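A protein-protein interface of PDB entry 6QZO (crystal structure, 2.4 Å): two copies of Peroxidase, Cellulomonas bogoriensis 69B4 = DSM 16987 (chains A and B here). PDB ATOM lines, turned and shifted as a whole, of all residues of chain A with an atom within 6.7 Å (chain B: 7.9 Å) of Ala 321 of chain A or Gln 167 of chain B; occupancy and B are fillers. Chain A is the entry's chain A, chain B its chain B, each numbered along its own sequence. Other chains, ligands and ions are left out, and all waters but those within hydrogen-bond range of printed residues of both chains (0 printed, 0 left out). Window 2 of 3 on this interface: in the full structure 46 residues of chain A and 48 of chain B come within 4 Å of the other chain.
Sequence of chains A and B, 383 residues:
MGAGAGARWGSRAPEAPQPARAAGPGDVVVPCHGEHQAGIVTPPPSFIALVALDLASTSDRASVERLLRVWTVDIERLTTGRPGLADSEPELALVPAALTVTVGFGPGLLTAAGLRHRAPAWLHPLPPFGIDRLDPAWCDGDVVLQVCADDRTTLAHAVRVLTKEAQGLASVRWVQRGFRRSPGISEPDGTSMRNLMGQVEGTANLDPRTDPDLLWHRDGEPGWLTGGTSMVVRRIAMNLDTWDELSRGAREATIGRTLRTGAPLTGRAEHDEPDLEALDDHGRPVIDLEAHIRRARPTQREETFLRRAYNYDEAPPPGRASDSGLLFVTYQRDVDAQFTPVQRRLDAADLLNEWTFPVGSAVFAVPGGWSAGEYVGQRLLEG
No position is printed for both chains.
Of the 12 pairs that touch across the chains among the printed residues, none has its exchanged pair printed and touching as well.
O of Asp 323 of chain A lies within hydrogen-bond range of N of Glu 314 of chain A, 2.7 Å away.
O of Ser 322 of chain A sits at hydrogen-bond distance from NH2 of Arg 320 of chain A, at 3.2 Å.
O of Val 159 of chain B is in hydrogen-bond range of OG1 of Thr 163 of chain B (2.6 Å).
Of the printed residues of chain B, Glu 314 of chain A touches Arg 177 (3.4 Å).
Of chain B, only Arg 160, Thr 163 and Gln 167 come within 4 Å of Ala 321 of chain A.
Printed residues of chain B within 4 Å of Ser 322 of chain A: Arg 160 (3.1 Å).
Printed residues of chain A within 4 Å of Thr 163 of chain B: Ala 321 (3.4 Å).
Of chain A, only Ala 321 comes within 4 Å of Gln 167 of chain B.
Printed residues of chain A within 4 Å of Arg 177 of chain B: Glu 314 and Ala 315.
The nearest residue of chain B that does not touch Ala 321 of chain A is Val 172 of chain B (4.4 Å).
Of the 22 printed residues of chain B, 7 touch a printed residue of chain A.
Hydrophobic or aromatic side chains of chain B within 4 Å of the printed part of chain A: Val 172 and Val 175.
Among the printed residues, Asp or Glu carboxylates within 4 Å of a Lys or Arg side-chain nitrogen of the other chain: Asp 241 of chain A with Arg 160 of chain B, Asp 244 of chain A with Arg 160 of chain B and Asp 244 of chain A with Lys 164 of chain B.
The side-chain carboxylate (OD1) of Asp 241 of chain A is in salt-bridge range of the guanidinium group (NH2) of Arg 160 of chain B (3.1 Å).
The side-chain carboxylate (OD2) of Asp 244 of chain A is in salt-bridge range of the guanidinium group (NH2) of Arg 160 of chain B, 3.0 Å away.
NZ of Lys 164 of chain B is in salt-bridge range of OD2 of Asp 244 of chain A, 2.9 Å away.
The guanidinium group of Arg 177 of chain B sits at hydrogen-bond distance from the backbone carbonyl oxygen of Glu 314 of chain A.
OG of Ser 322 of chain A is in hydrogen-bond range of NH1 of Arg 160 of chain B, at 3.1 Å.
NE of Arg 177 of chain B lies close to N of Ala 315 of chain A, at 3.3 Å.
Among the printed residues, pairs that only touch across the chains: Ala 315 of chain A with Val 175 of chain B (3.7 Å), Pro 316 of chain A with Val 172 of chain B (3.98 Å), Pro 316 of chain A with Val 175 of chain B (3.6 Å), Ala 321 of chain A with Arg 160 of chain B (3.95 Å), Ala 321 of chain A with Thr 163 of chain B (3.4 Å) and Ala 321 of chain A with Gln 167 of chain B (3.9 Å).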
ATOM      1  N   ASP A 241       8.482  28.915 -17.988  1.00  0.00           N
ATOM      2  CA  ASP A 241       9.971  28.902 -17.980  1.00  0.00           C
ATOM      3  C   ASP A 241      10.490  28.944 -16.536  1.00  0.00           C
ATOM      4  O   ASP A 241      11.358  28.118 -16.231  1.00  0.00           O
ATOM      5  CB  ASP A 241      10.569  30.035 -18.819  1.00  0.00           C
ATOM      6  CG  ASP A 241      10.314  29.915 -20.307  1.00  0.00           C
ATOM      7  OD1 ASP A 241      10.017  28.795 -20.777  1.00  0.00           O
ATOM      8  OD2 ASP A 241      10.415  30.944 -20.987  1.00  0.00           O
ATOM      9  N   ASP A 244       9.369  25.840 -14.332  1.00  0.00           N
ATOM     10  CA  ASP A 244      10.245  24.669 -14.619  1.00  0.00           C
ATOM     11  C   ASP A 244      11.424  24.602 -13.636  1.00  0.00           C
ATOM     12  O   ASP A 244      11.985  23.505 -13.489  1.00  0.00           O
ATOM     13  CB  ASP A 244      10.712  24.687 -16.074  1.00  0.00           C
ATOM     14  CG  ASP A 244       9.642  24.242 -17.036  1.00  0.00           C
ATOM     15  OD1 ASP A 244       8.535  23.876 -16.556  1.00  0.00           O
ATOM     16  OD2 ASP A 244       9.925  24.271 -18.258  1.00  0.00           O
ATOM     17  N   GLU A 314      -1.061  29.878 -27.071  1.00  0.00           N
ATOM     18  CA  GLU A 314      -0.987  30.688 -28.318  1.00  0.00           C
ATOM     19  C   GLU A 314       0.335  30.435 -29.022  1.00  0.00           C
ATOM     20  O   GLU A 314       1.278  30.032 -28.344  1.00  0.00           O
ATOM     21  CB  GLU A 314      -1.129  32.190 -28.005  1.00  0.00           C
ATOM     22  CG  GLU A 314      -2.459  32.556 -27.397  1.00  0.00           C
ATOM     23  CD  GLU A 314      -3.677  32.040 -28.150  1.00  0.00           C
ATOM     24  OE1 GLU A 314      -3.670  31.989 -29.390  1.00  0.00           O
ATOM     25  OE2 GLU A 314      -4.628  31.671 -27.485  1.00  0.00           O
ATOM     26  N   ALA A 315       0.392  30.696 -30.325  1.00  0.00           N
ATOM     27  CA  ALA A 315       1.661  30.853 -31.060  1.00  0.00           C
ATOM     28  C   ALA A 315       2.494  31.829 -30.245  1.00  0.00           C
ATOM     29  O   ALA A 315       2.012  32.918 -29.933  1.00  0.00           O
ATOM     30  CB  ALA A 315       1.412  31.343 -32.460  1.00  0.00           C
ATOM     31  N   PRO A 316       3.710  31.450 -29.786  1.00  0.00           N
ATOM     32  CA  PRO A 316       4.487  32.312 -28.898  1.00  0.00           C
ATOM     33  C   PRO A 316       5.029  33.569 -29.574  1.00  0.00           C
ATOM     34  O   PRO A 316       5.294  33.570 -30.772  1.00  0.00           O
ATOM     35  CB  PRO A 316       5.642  31.395 -28.461  1.00  0.00           C
ATOM     36  CG  PRO A 316       5.805  30.462 -29.639  1.00  0.00           C
ATOM     37  CD  PRO A 316       4.386  30.177 -30.070  1.00  0.00           C
ATOM     38  N   PRO A 317       5.296  34.648 -28.801  1.00  0.00           N
ATOM     39  CA  PRO A 317       5.891  35.864 -29.354  1.00  0.00           C
ATOM     40  C   PRO A 317       7.349  35.601 -29.713  1.00  0.00           C
ATOM     41  O   PRO A 317       7.922  34.596 -29.293  1.00  0.00           O
ATOM     42  CB  PRO A 317       5.767  36.881 -28.213  1.00  0.00           C
ATOM     43  CG  PRO A 317       5.821  36.009 -26.955  1.00  0.00           C
ATOM     44  CD  PRO A 317       5.102  34.726 -27.340  1.00  0.00           C
ATOM     45  N   PRO A 318       7.996  36.500 -30.493  1.00  0.00           N
ATOM     46  CA  PRO A 318       9.313  36.219 -31.065  1.00  0.00           C
ATOM     47  C   PRO A 318      10.348  35.521 -30.174  1.00  0.00           C
ATOM     48  O   PRO A 318      10.919  34.587 -30.702  1.00  0.00           O
ATOM     49  CB  PRO A 318       9.807  37.607 -31.489  1.00  0.00           C
ATOM     50  CG  PRO A 318       8.526  38.317 -31.899  1.00  0.00           C
ATOM     51  CD  PRO A 318       7.483  37.809 -30.926  1.00  0.00           C
ATOM     52  N   GLY A 319      10.582  35.929 -28.915  1.00  0.00           N
ATOM     53  CA  GLY A 319      11.755  35.440 -28.160  1.00  0.00           C
ATOM     54  C   GLY A 319      11.510  34.145 -27.387  1.00  0.00           C
ATOM     55  O   GLY A 319      12.470  33.643 -26.790  1.00  0.00           O
ATOM     56  N   ARG A 320      10.272  33.637 -27.359  1.00  0.00           N
ATOM     57  CA  ARG A 320       9.797  32.713 -26.293  1.00  0.00           C
ATOM     58  C   ARG A 320       9.386  31.353 -26.864  1.00  0.00           C
ATOM     59  O   ARG A 320       9.013  31.282 -28.053  1.00  0.00           O
ATOM     60  CB  ARG A 320       8.621  33.356 -25.557  1.00  0.00           C
ATOM     61  CG  ARG A 320       8.878  34.772 -25.051  1.00  0.00           C
ATOM     62  CD  ARG A 320       8.221  35.047 -23.705  1.00  0.00           C
ATOM     63  NE  ARG A 320       6.788  34.744 -23.784  1.00  0.00           N
ATOM     64  CZ  ARG A 320       5.956  34.574 -22.760  1.00  0.00           C
ATOM     65  NH1 ARG A 320       6.370  34.700 -21.509  1.00  0.00           N
ATOM     66  NH2 ARG A 320       4.684  34.269 -22.992  1.00  0.00           N
ATOM     67  N   ALA A 321       9.446  30.318 -26.026  1.00  0.00           N
ATOM     68  CA  ALA A 321       9.048  28.925 -26.347  1.00  0.00           C
ATOM     69  C   ALA A 321       7.519  28.797 -26.368  1.00  0.00           C
ATOM     70  O   ALA A 321       6.984  28.111 -27.257  1.00  0.00           O
ATOM     71  CB  ALA A 321       9.667  27.983 -25.341  1.00  0.00           C
ATOM     72  N   SER A 322       6.844  29.417 -25.408  1.00  0.00           N
ATOM     73  CA  SER A 322       5.391  29.205 -25.150  1.00  0.00           C
ATOM     74  C   SER A 322       4.709  30.527 -24.781  1.00  0.00           C
ATOM     75  O   SER A 322       5.365  31.406 -24.208  1.00  0.00           O
ATOM     76  CB  SER A 322       5.182  28.160 -24.068  1.00  0.00           C
ATOM     77  OG  SER A 322       5.846  26.943 -24.375  1.00  0.00           O
ATOM     78  N   ASP A 323       3.426  30.645 -25.106  1.00  0.00           N
ATOM     79  CA  ASP A 323       2.483  31.643 -24.552  1.00  0.00           C
ATOM     80  C   ASP A 323       1.273  30.859 -24.054  1.00  0.00           C
ATOM     81  O   ASP A 323       0.312  30.688 -24.837  1.00  0.00           O
ATOM     82  CB  ASP A 323       2.124  32.740 -25.564  1.00  0.00           C
ATOM     83  CG  ASP A 323       1.196  33.820 -24.990  1.00  0.00           C
ATOM     84  OD1 ASP A 323       0.937  33.789 -23.773  1.00  0.00           O
ATOM     85  OD2 ASP A 323       0.762  34.693 -25.731  1.00  0.00           O
ATOM     86  N   VAL B  51       5.556  23.429 -35.975  1.00  0.00           N
ATOM     87  CA  VAL B  51       6.552  24.270 -35.261  1.00  0.00           C
ATOM     88  C   VAL B  51       7.823  24.315 -36.118  1.00  0.00           C
ATOM     89  O   VAL B  51       8.547  23.320 -36.179  1.00  0.00           O
ATOM     90  CB  VAL B  51       6.834  23.748 -33.843  1.00  0.00           C
ATOM     91  CG1 VAL B  51       7.736  24.701 -33.086  1.00  0.00           C
ATOM     92  CG2 VAL B  51       5.542  23.458 -33.075  1.00  0.00           C
ATOM     93  N   LEU B  53      11.508  25.831 -36.441  1.00  0.00           N
ATOM     94  CA  LEU B  53      12.593  26.325 -35.568  1.00  0.00           C
ATOM     95  C   LEU B  53      13.757  26.753 -36.450  1.00  0.00           C
ATOM     96  O   LEU B  53      13.878  26.224 -37.575  1.00  0.00           O
ATOM     97  CB  LEU B  53      12.983  25.230 -34.579  1.00  0.00           C
ATOM     98  CG  LEU B  53      11.871  24.741 -33.659  1.00  0.00           C
ATOM     99  CD1 LEU B  53      11.295  23.438 -34.183  1.00  0.00           C
ATOM    100  CD2 LEU B  53      12.399  24.562 -32.237  1.00  0.00           C
ATOM    101  N   ALA B  56      20.565  27.779 -33.810  1.00  0.00           N
ATOM    102  CA  ALA B  56      21.435  28.795 -33.176  1.00  0.00           C
ATOM    103  C   ALA B  56      22.598  29.113 -34.126  1.00  0.00           C
ATOM    104  O   ALA B  56      22.981  28.244 -34.917  1.00  0.00           O
ATOM    105  CB  ALA B  56      21.944  28.307 -31.844  1.00  0.00           C
ATOM    106  N   LEU B  67      20.433  17.450 -31.185  1.00  0.00           N
ATOM    107  CA  LEU B  67      19.026  17.902 -31.249  1.00  0.00           C
ATOM    108  C   LEU B  67      18.116  16.771 -31.734  1.00  0.00           C
ATOM    109  O   LEU B  67      17.093  16.497 -31.081  1.00  0.00           O
ATOM    110  CB  LEU B  67      18.943  19.108 -32.187  1.00  0.00           C
ATOM    111  CG  LEU B  67      17.545  19.657 -32.420  1.00  0.00           C
ATOM    112  CD1 LEU B  67      16.932  20.077 -31.106  1.00  0.00           C
ATOM    113  CD2 LEU B  67      17.587  20.823 -33.397  1.00  0.00           C
ATOM    114  N   VAL B  70      17.946  13.871 -29.028  1.00  0.00           N
ATOM    115  CA  VAL B  70      17.099  14.161 -27.841  1.00  0.00           C
ATOM    116  C   VAL B  70      15.628  14.152 -28.281  1.00  0.00           C
ATOM    117  O   VAL B  70      14.781  13.630 -27.516  1.00  0.00           O
ATOM    118  CB  VAL B  70      17.492  15.455 -27.106  1.00  0.00           C
ATOM    119  CG1 VAL B  70      18.881  15.349 -26.490  1.00  0.00           C
ATOM    120  CG2 VAL B  70      17.409  16.686 -27.983  1.00  0.00           C
ATOM    121  N   TRP B  71      15.322  14.666 -29.474  1.00  0.00           N
ATOM    122  CA  TRP B  71      13.938  14.677 -30.025  1.00  0.00           C
ATOM    123  C   TRP B  71      13.449  13.248 -30.247  1.00  0.00           C
ATOM    124  O   TRP B  71      12.268  12.969 -29.964  1.00  0.00           O
ATOM    125  CB  TRP B  71      13.858  15.482 -31.321  1.00  0.00           C
ATOM    126  CG  TRP B  71      13.643  16.941 -31.121  1.00  0.00           C
ATOM    127  CD1 TRP B  71      13.279  17.582 -29.968  1.00  0.00           C
ATOM    128  CD2 TRP B  71      13.731  17.959 -32.132  1.00  0.00           C
ATOM    129  NE1 TRP B  71      13.168  18.931 -30.189  1.00  0.00           N
ATOM    130  CE2 TRP B  71      13.415  19.188 -31.511  1.00  0.00           C
ATOM    131  CE3 TRP B  71      14.066  17.948 -33.487  1.00  0.00           C
ATOM    132  CZ2 TRP B  71      13.420  20.388 -32.212  1.00  0.00           C
ATOM    133  CZ3 TRP B  71      14.072  19.133 -34.172  1.00  0.00           C
ATOM    134  CH2 TRP B  71      13.754  20.340 -33.538  1.00  0.00           C
ATOM    135  N   VAL B 159       4.357  19.817 -27.735  1.00  0.00           N
ATOM    136  CA  VAL B 159       5.001  21.037 -28.299  1.00  0.00           C
ATOM    137  C   VAL B 159       5.905  21.663 -27.228  1.00  0.00           C
ATOM    138  O   VAL B 159       7.051  22.060 -27.564  1.00  0.00           O
ATOM    139  CB  VAL B 159       3.940  22.030 -28.814  1.00  0.00           C
ATOM    140  CG1 VAL B 159       4.511  23.427 -29.049  1.00  0.00           C
ATOM    141  CG2 VAL B 159       3.261  21.502 -30.081  1.00  0.00           C
ATOM    142  N   ARG B 160       5.425  21.779 -25.994  1.00  0.00           N
ATOM    143  CA  ARG B 160       6.200  22.384 -24.875  1.00  0.00           C
ATOM    144  C   ARG B 160       7.469  21.544 -24.651  1.00  0.00           C
ATOM    145  O   ARG B 160       8.554  22.123 -24.511  1.00  0.00           O
ATOM    146  CB  ARG B 160       5.309  22.478 -23.624  1.00  0.00           C
ATOM    147  CG  ARG B 160       6.011  22.885 -22.334  1.00  0.00           C
ATOM    148  CD  ARG B 160       6.418  24.340 -22.342  1.00  0.00           C
ATOM    149  NE  ARG B 160       7.129  24.777 -21.140  1.00  0.00           N
ATOM    150  CZ  ARG B 160       7.790  25.926 -21.033  1.00  0.00           C
ATOM    151  NH1 ARG B 160       7.848  26.771 -22.049  1.00  0.00           N
ATOM    152  NH2 ARG B 160       8.425  26.224 -19.920  1.00  0.00           N
ATOM    153  N   VAL B 161       7.352  20.220 -24.613  1.00  0.00           N
ATOM    154  CA  VAL B 161       8.495  19.303 -24.322  1.00  0.00           C
ATOM    155  C   VAL B 161       9.509  19.403 -25.460  1.00  0.00           C
ATOM    156  O   VAL B 161      10.703  19.595 -25.164  1.00  0.00           O
ATOM    157  CB  VAL B 161       8.025  17.859 -24.086  1.00  0.00           C
ATOM    158  CG1 VAL B 161       9.203  16.876 -24.094  1.00  0.00           C
ATOM    159  CG2 VAL B 161       7.265  17.766 -22.765  1.00  0.00           C
ATOM    160  N   LEU B 162       9.069  19.287 -26.707  1.00  0.00           N
ATOM    161  CA  LEU B 162       9.991  19.279 -27.881  1.00  0.00           C
ATOM    162  C   LEU B 162      10.692  20.632 -27.989  1.00  0.00           C
ATOM    163  O   LEU B 162      11.875  20.646 -28.308  1.00  0.00           O
ATOM    164  CB  LEU B 162       9.209  18.931 -29.144  1.00  0.00           C
ATOM    165  CG  LEU B 162       8.646  17.515 -29.130  1.00  0.00           C
ATOM    166  CD1 LEU B 162       7.566  17.350 -30.178  1.00  0.00           C
ATOM    167  CD2 LEU B 162       9.738  16.487 -29.346  1.00  0.00           C
ATOM    168  N   THR B 163       9.976  21.723 -27.709  1.00  0.00           N
ATOM    169  CA  THR B 163      10.497  23.116 -27.798  1.00  0.00           C
ATOM    170  C   THR B 163      11.581  23.304 -26.736  1.00  0.00           C
ATOM    171  O   THR B 163      12.660  23.790 -27.078  1.00  0.00           O
ATOM    172  CB  THR B 163       9.367  24.145 -27.662  1.00  0.00           C
ATOM    173  OG1 THR B 163       8.443  23.884 -28.713  1.00  0.00           O
ATOM    174  CG2 THR B 163       9.851  25.575 -27.777  1.00  0.00           C
ATOM    175  N   LYS B 164      11.292  22.934 -25.490  1.00  0.00           N
ATOM    176  CA  LYS B 164      12.249  22.994 -24.354  1.00  0.00           C
ATOM    177  C   LYS B 164      13.512  22.181 -24.665  1.00  0.00           C
ATOM    178  O   LYS B 164      14.599  22.622 -24.297  1.00  0.00           O
ATOM    179  CB  LYS B 164      11.601  22.436 -23.087  1.00  0.00           C
ATOM    180  CG  LYS B 164      10.737  23.419 -22.318  1.00  0.00           C
ATOM    181  CD  LYS B 164       9.894  22.757 -21.226  1.00  0.00           C
ATOM    182  CE  LYS B 164      10.770  22.126 -20.157  1.00  0.00           C
ATOM    183  NZ  LYS B 164       9.994  21.521 -19.047  1.00  0.00           N
ATOM    184  N   GLU B 165      13.362  21.007 -25.271  1.00  0.00           N
ATOM    185  CA  GLU B 165      14.492  20.084 -25.558  1.00  0.00           C
ATOM    186  C   GLU B 165      15.503  20.759 -26.499  1.00  0.00           C
ATOM    187  O   GLU B 165      16.706  20.463 -26.370  1.00  0.00           O
ATOM    188  CB  GLU B 165      13.979  18.807 -26.202  1.00  0.00           C
ATOM    189  CG  GLU B 165      14.859  17.624 -25.922  1.00  0.00           C
ATOM    190  CD  GLU B 165      14.826  17.248 -24.453  1.00  0.00           C
ATOM    191  OE1 GLU B 165      13.790  16.693 -24.018  1.00  0.00           O
ATOM    192  OE2 GLU B 165      15.804  17.537 -23.744  1.00  0.00           O
ATOM    193  N   ALA B 166      15.020  21.629 -27.395  1.00  0.00           N
ATOM    194  CA  ALA B 166      15.833  22.320 -28.418  1.00  0.00           C
ATOM    195  C   ALA B 166      16.452  23.611 -27.855  1.00  0.00           C
ATOM    196  O   ALA B 166      17.190  24.268 -28.602  1.00  0.00           O
ATOM    197  CB  ALA B 166      14.972  22.615 -29.616  1.00  0.00           C
ATOM    198  N   GLN B 167      16.180  23.956 -26.597  1.00  0.00           N
ATOM    199  CA  GLN B 167      16.665  25.226 -25.977  1.00  0.00           C
ATOM    200  C   GLN B 167      18.192  25.264 -26.129  1.00  0.00           C
ATOM    201  O   GLN B 167      18.863  24.279 -25.708  1.00  0.00           O
ATOM    202  CB  GLN B 167      16.215  25.365 -24.516  1.00  0.00           C
ATOM    203  CG  GLN B 167      15.756  26.784 -24.163  1.00  0.00           C
ATOM    204  CD  GLN B 167      14.257  26.870 -23.912  1.00  0.00           C
ATOM    205  OE1 GLN B 167      13.774  26.407 -22.884  1.00  0.00           O
ATOM    206  NE2 GLN B 167      13.493  27.498 -24.806  1.00  0.00           N
ATOM    207  N   GLY B 168      18.723  26.323 -26.758  1.00  0.00           N
ATOM    208  CA  GLY B 168      20.174  26.480 -27.006  1.00  0.00           C
ATOM    209  C   GLY B 168      20.654  25.867 -28.323  1.00  0.00           C
ATOM    210  O   GLY B 168      21.785  26.196 -28.727  1.00  0.00           O
ATOM    211  N   LEU B 169      19.848  25.020 -28.969  1.00  0.00           N
ATOM    212  CA  LEU B 169      20.181  24.345 -30.265  1.00  0.00           C
ATOM    213  C   LEU B 169      19.347  24.924 -31.401  1.00  0.00           C
ATOM    214  O   LEU B 169      19.870  25.059 -32.518  1.00  0.00           O
ATOM    215  CB  LEU B 169      19.941  22.832 -30.138  1.00  0.00           C
ATOM    216  CG  LEU B 169      20.667  22.160 -28.977  1.00  0.00           C
ATOM    217  CD1 LEU B 169      20.133  20.767 -28.723  1.00  0.00           C
ATOM    218  CD2 LEU B 169      22.149  22.121 -29.245  1.00  0.00           C
ATOM    219  N   ALA B 170      18.088  25.241 -31.116  1.00  0.00           N
ATOM    220  CA  ALA B 170      17.151  25.870 -32.073  1.00  0.00           C
ATOM    221  C   ALA B 170      16.092  26.637 -31.293  1.00  0.00           C
ATOM    222  O   ALA B 170      15.756  26.199 -30.199  1.00  0.00           O
ATOM    223  CB  ALA B 170      16.530  24.823 -32.954  1.00  0.00           C
ATOM    224  N   SER B 171      15.606  27.737 -31.855  1.00  0.00           N
ATOM    225  CA  SER B 171      14.519  28.566 -31.277  1.00  0.00           C
ATOM    226  C   SER B 171      13.339  28.613 -32.251  1.00  0.00           C
ATOM    227  O   SER B 171      13.543  28.386 -33.455  1.00  0.00           O
ATOM    228  CB  SER B 171      15.033  29.935 -30.922  1.00  0.00           C
ATOM    229  OG  SER B 171      15.498  30.606 -32.069  1.00  0.00           O
ATOM    230  N   VAL B 172      12.141  28.839 -31.726  1.00  0.00           N
ATOM    231  CA  VAL B 172      10.870  28.849 -32.515  1.00  0.00           C
ATOM    232  C   VAL B 172      10.912  30.020 -33.496  1.00  0.00           C
ATOM    233  O   VAL B 172      11.284  31.115 -33.091  1.00  0.00           O
ATOM    234  CB  VAL B 172       9.641  28.906 -31.601  1.00  0.00           C
ATOM    235  CG1 VAL B 172       8.352  29.125 -32.394  1.00  0.00           C
ATOM    236  CG2 VAL B 172       9.555  27.633 -30.746  1.00  0.00           C
ATOM    237  N   VAL B 175       4.738  29.019 -35.381  1.00  0.00           N
ATOM    238  CA  VAL B 175       3.824  27.896 -35.036  1.00  0.00           C
ATOM    239  C   VAL B 175       2.500  28.163 -35.738  1.00  0.00           C
ATOM    240  O   VAL B 175       1.913  29.225 -35.510  1.00  0.00           O
ATOM    241  CB  VAL B 175       3.602  27.770 -33.524  1.00  0.00           C
ATOM    242  CG1 VAL B 175       2.784  26.532 -33.193  1.00  0.00           C
ATOM    243  CG2 VAL B 175       4.909  27.770 -32.755  1.00  0.00           C
ATOM    244  N   ARG B 177      -1.260  26.495 -36.117  1.00  0.00           N
ATOM    245  CA  ARG B 177      -2.180  25.581 -35.383  1.00  0.00           C
ATOM    246  C   ARG B 177      -3.391  25.379 -36.287  1.00  0.00           C
ATOM    247  O   ARG B 177      -3.827  26.362 -36.922  1.00  0.00           O
ATOM    248  CB  ARG B 177      -2.559  26.176 -34.019  1.00  0.00           C
ATOM    249  CG  ARG B 177      -1.390  26.889 -33.332  1.00  0.00           C
ATOM    250  CD  ARG B 177      -1.746  27.545 -32.005  1.00  0.00           C
ATOM    251  NE  ARG B 177      -0.566  27.678 -31.153  1.00  0.00           N
ATOM    252  CZ  ARG B 177       0.054  26.672 -30.514  1.00  0.00           C
ATOM    253  NH1 ARG B 177       1.130  26.937 -29.787  1.00  0.00           N
ATOM    254  NH2 ARG B 177      -0.401  25.422 -30.593  1.00  0.00           N
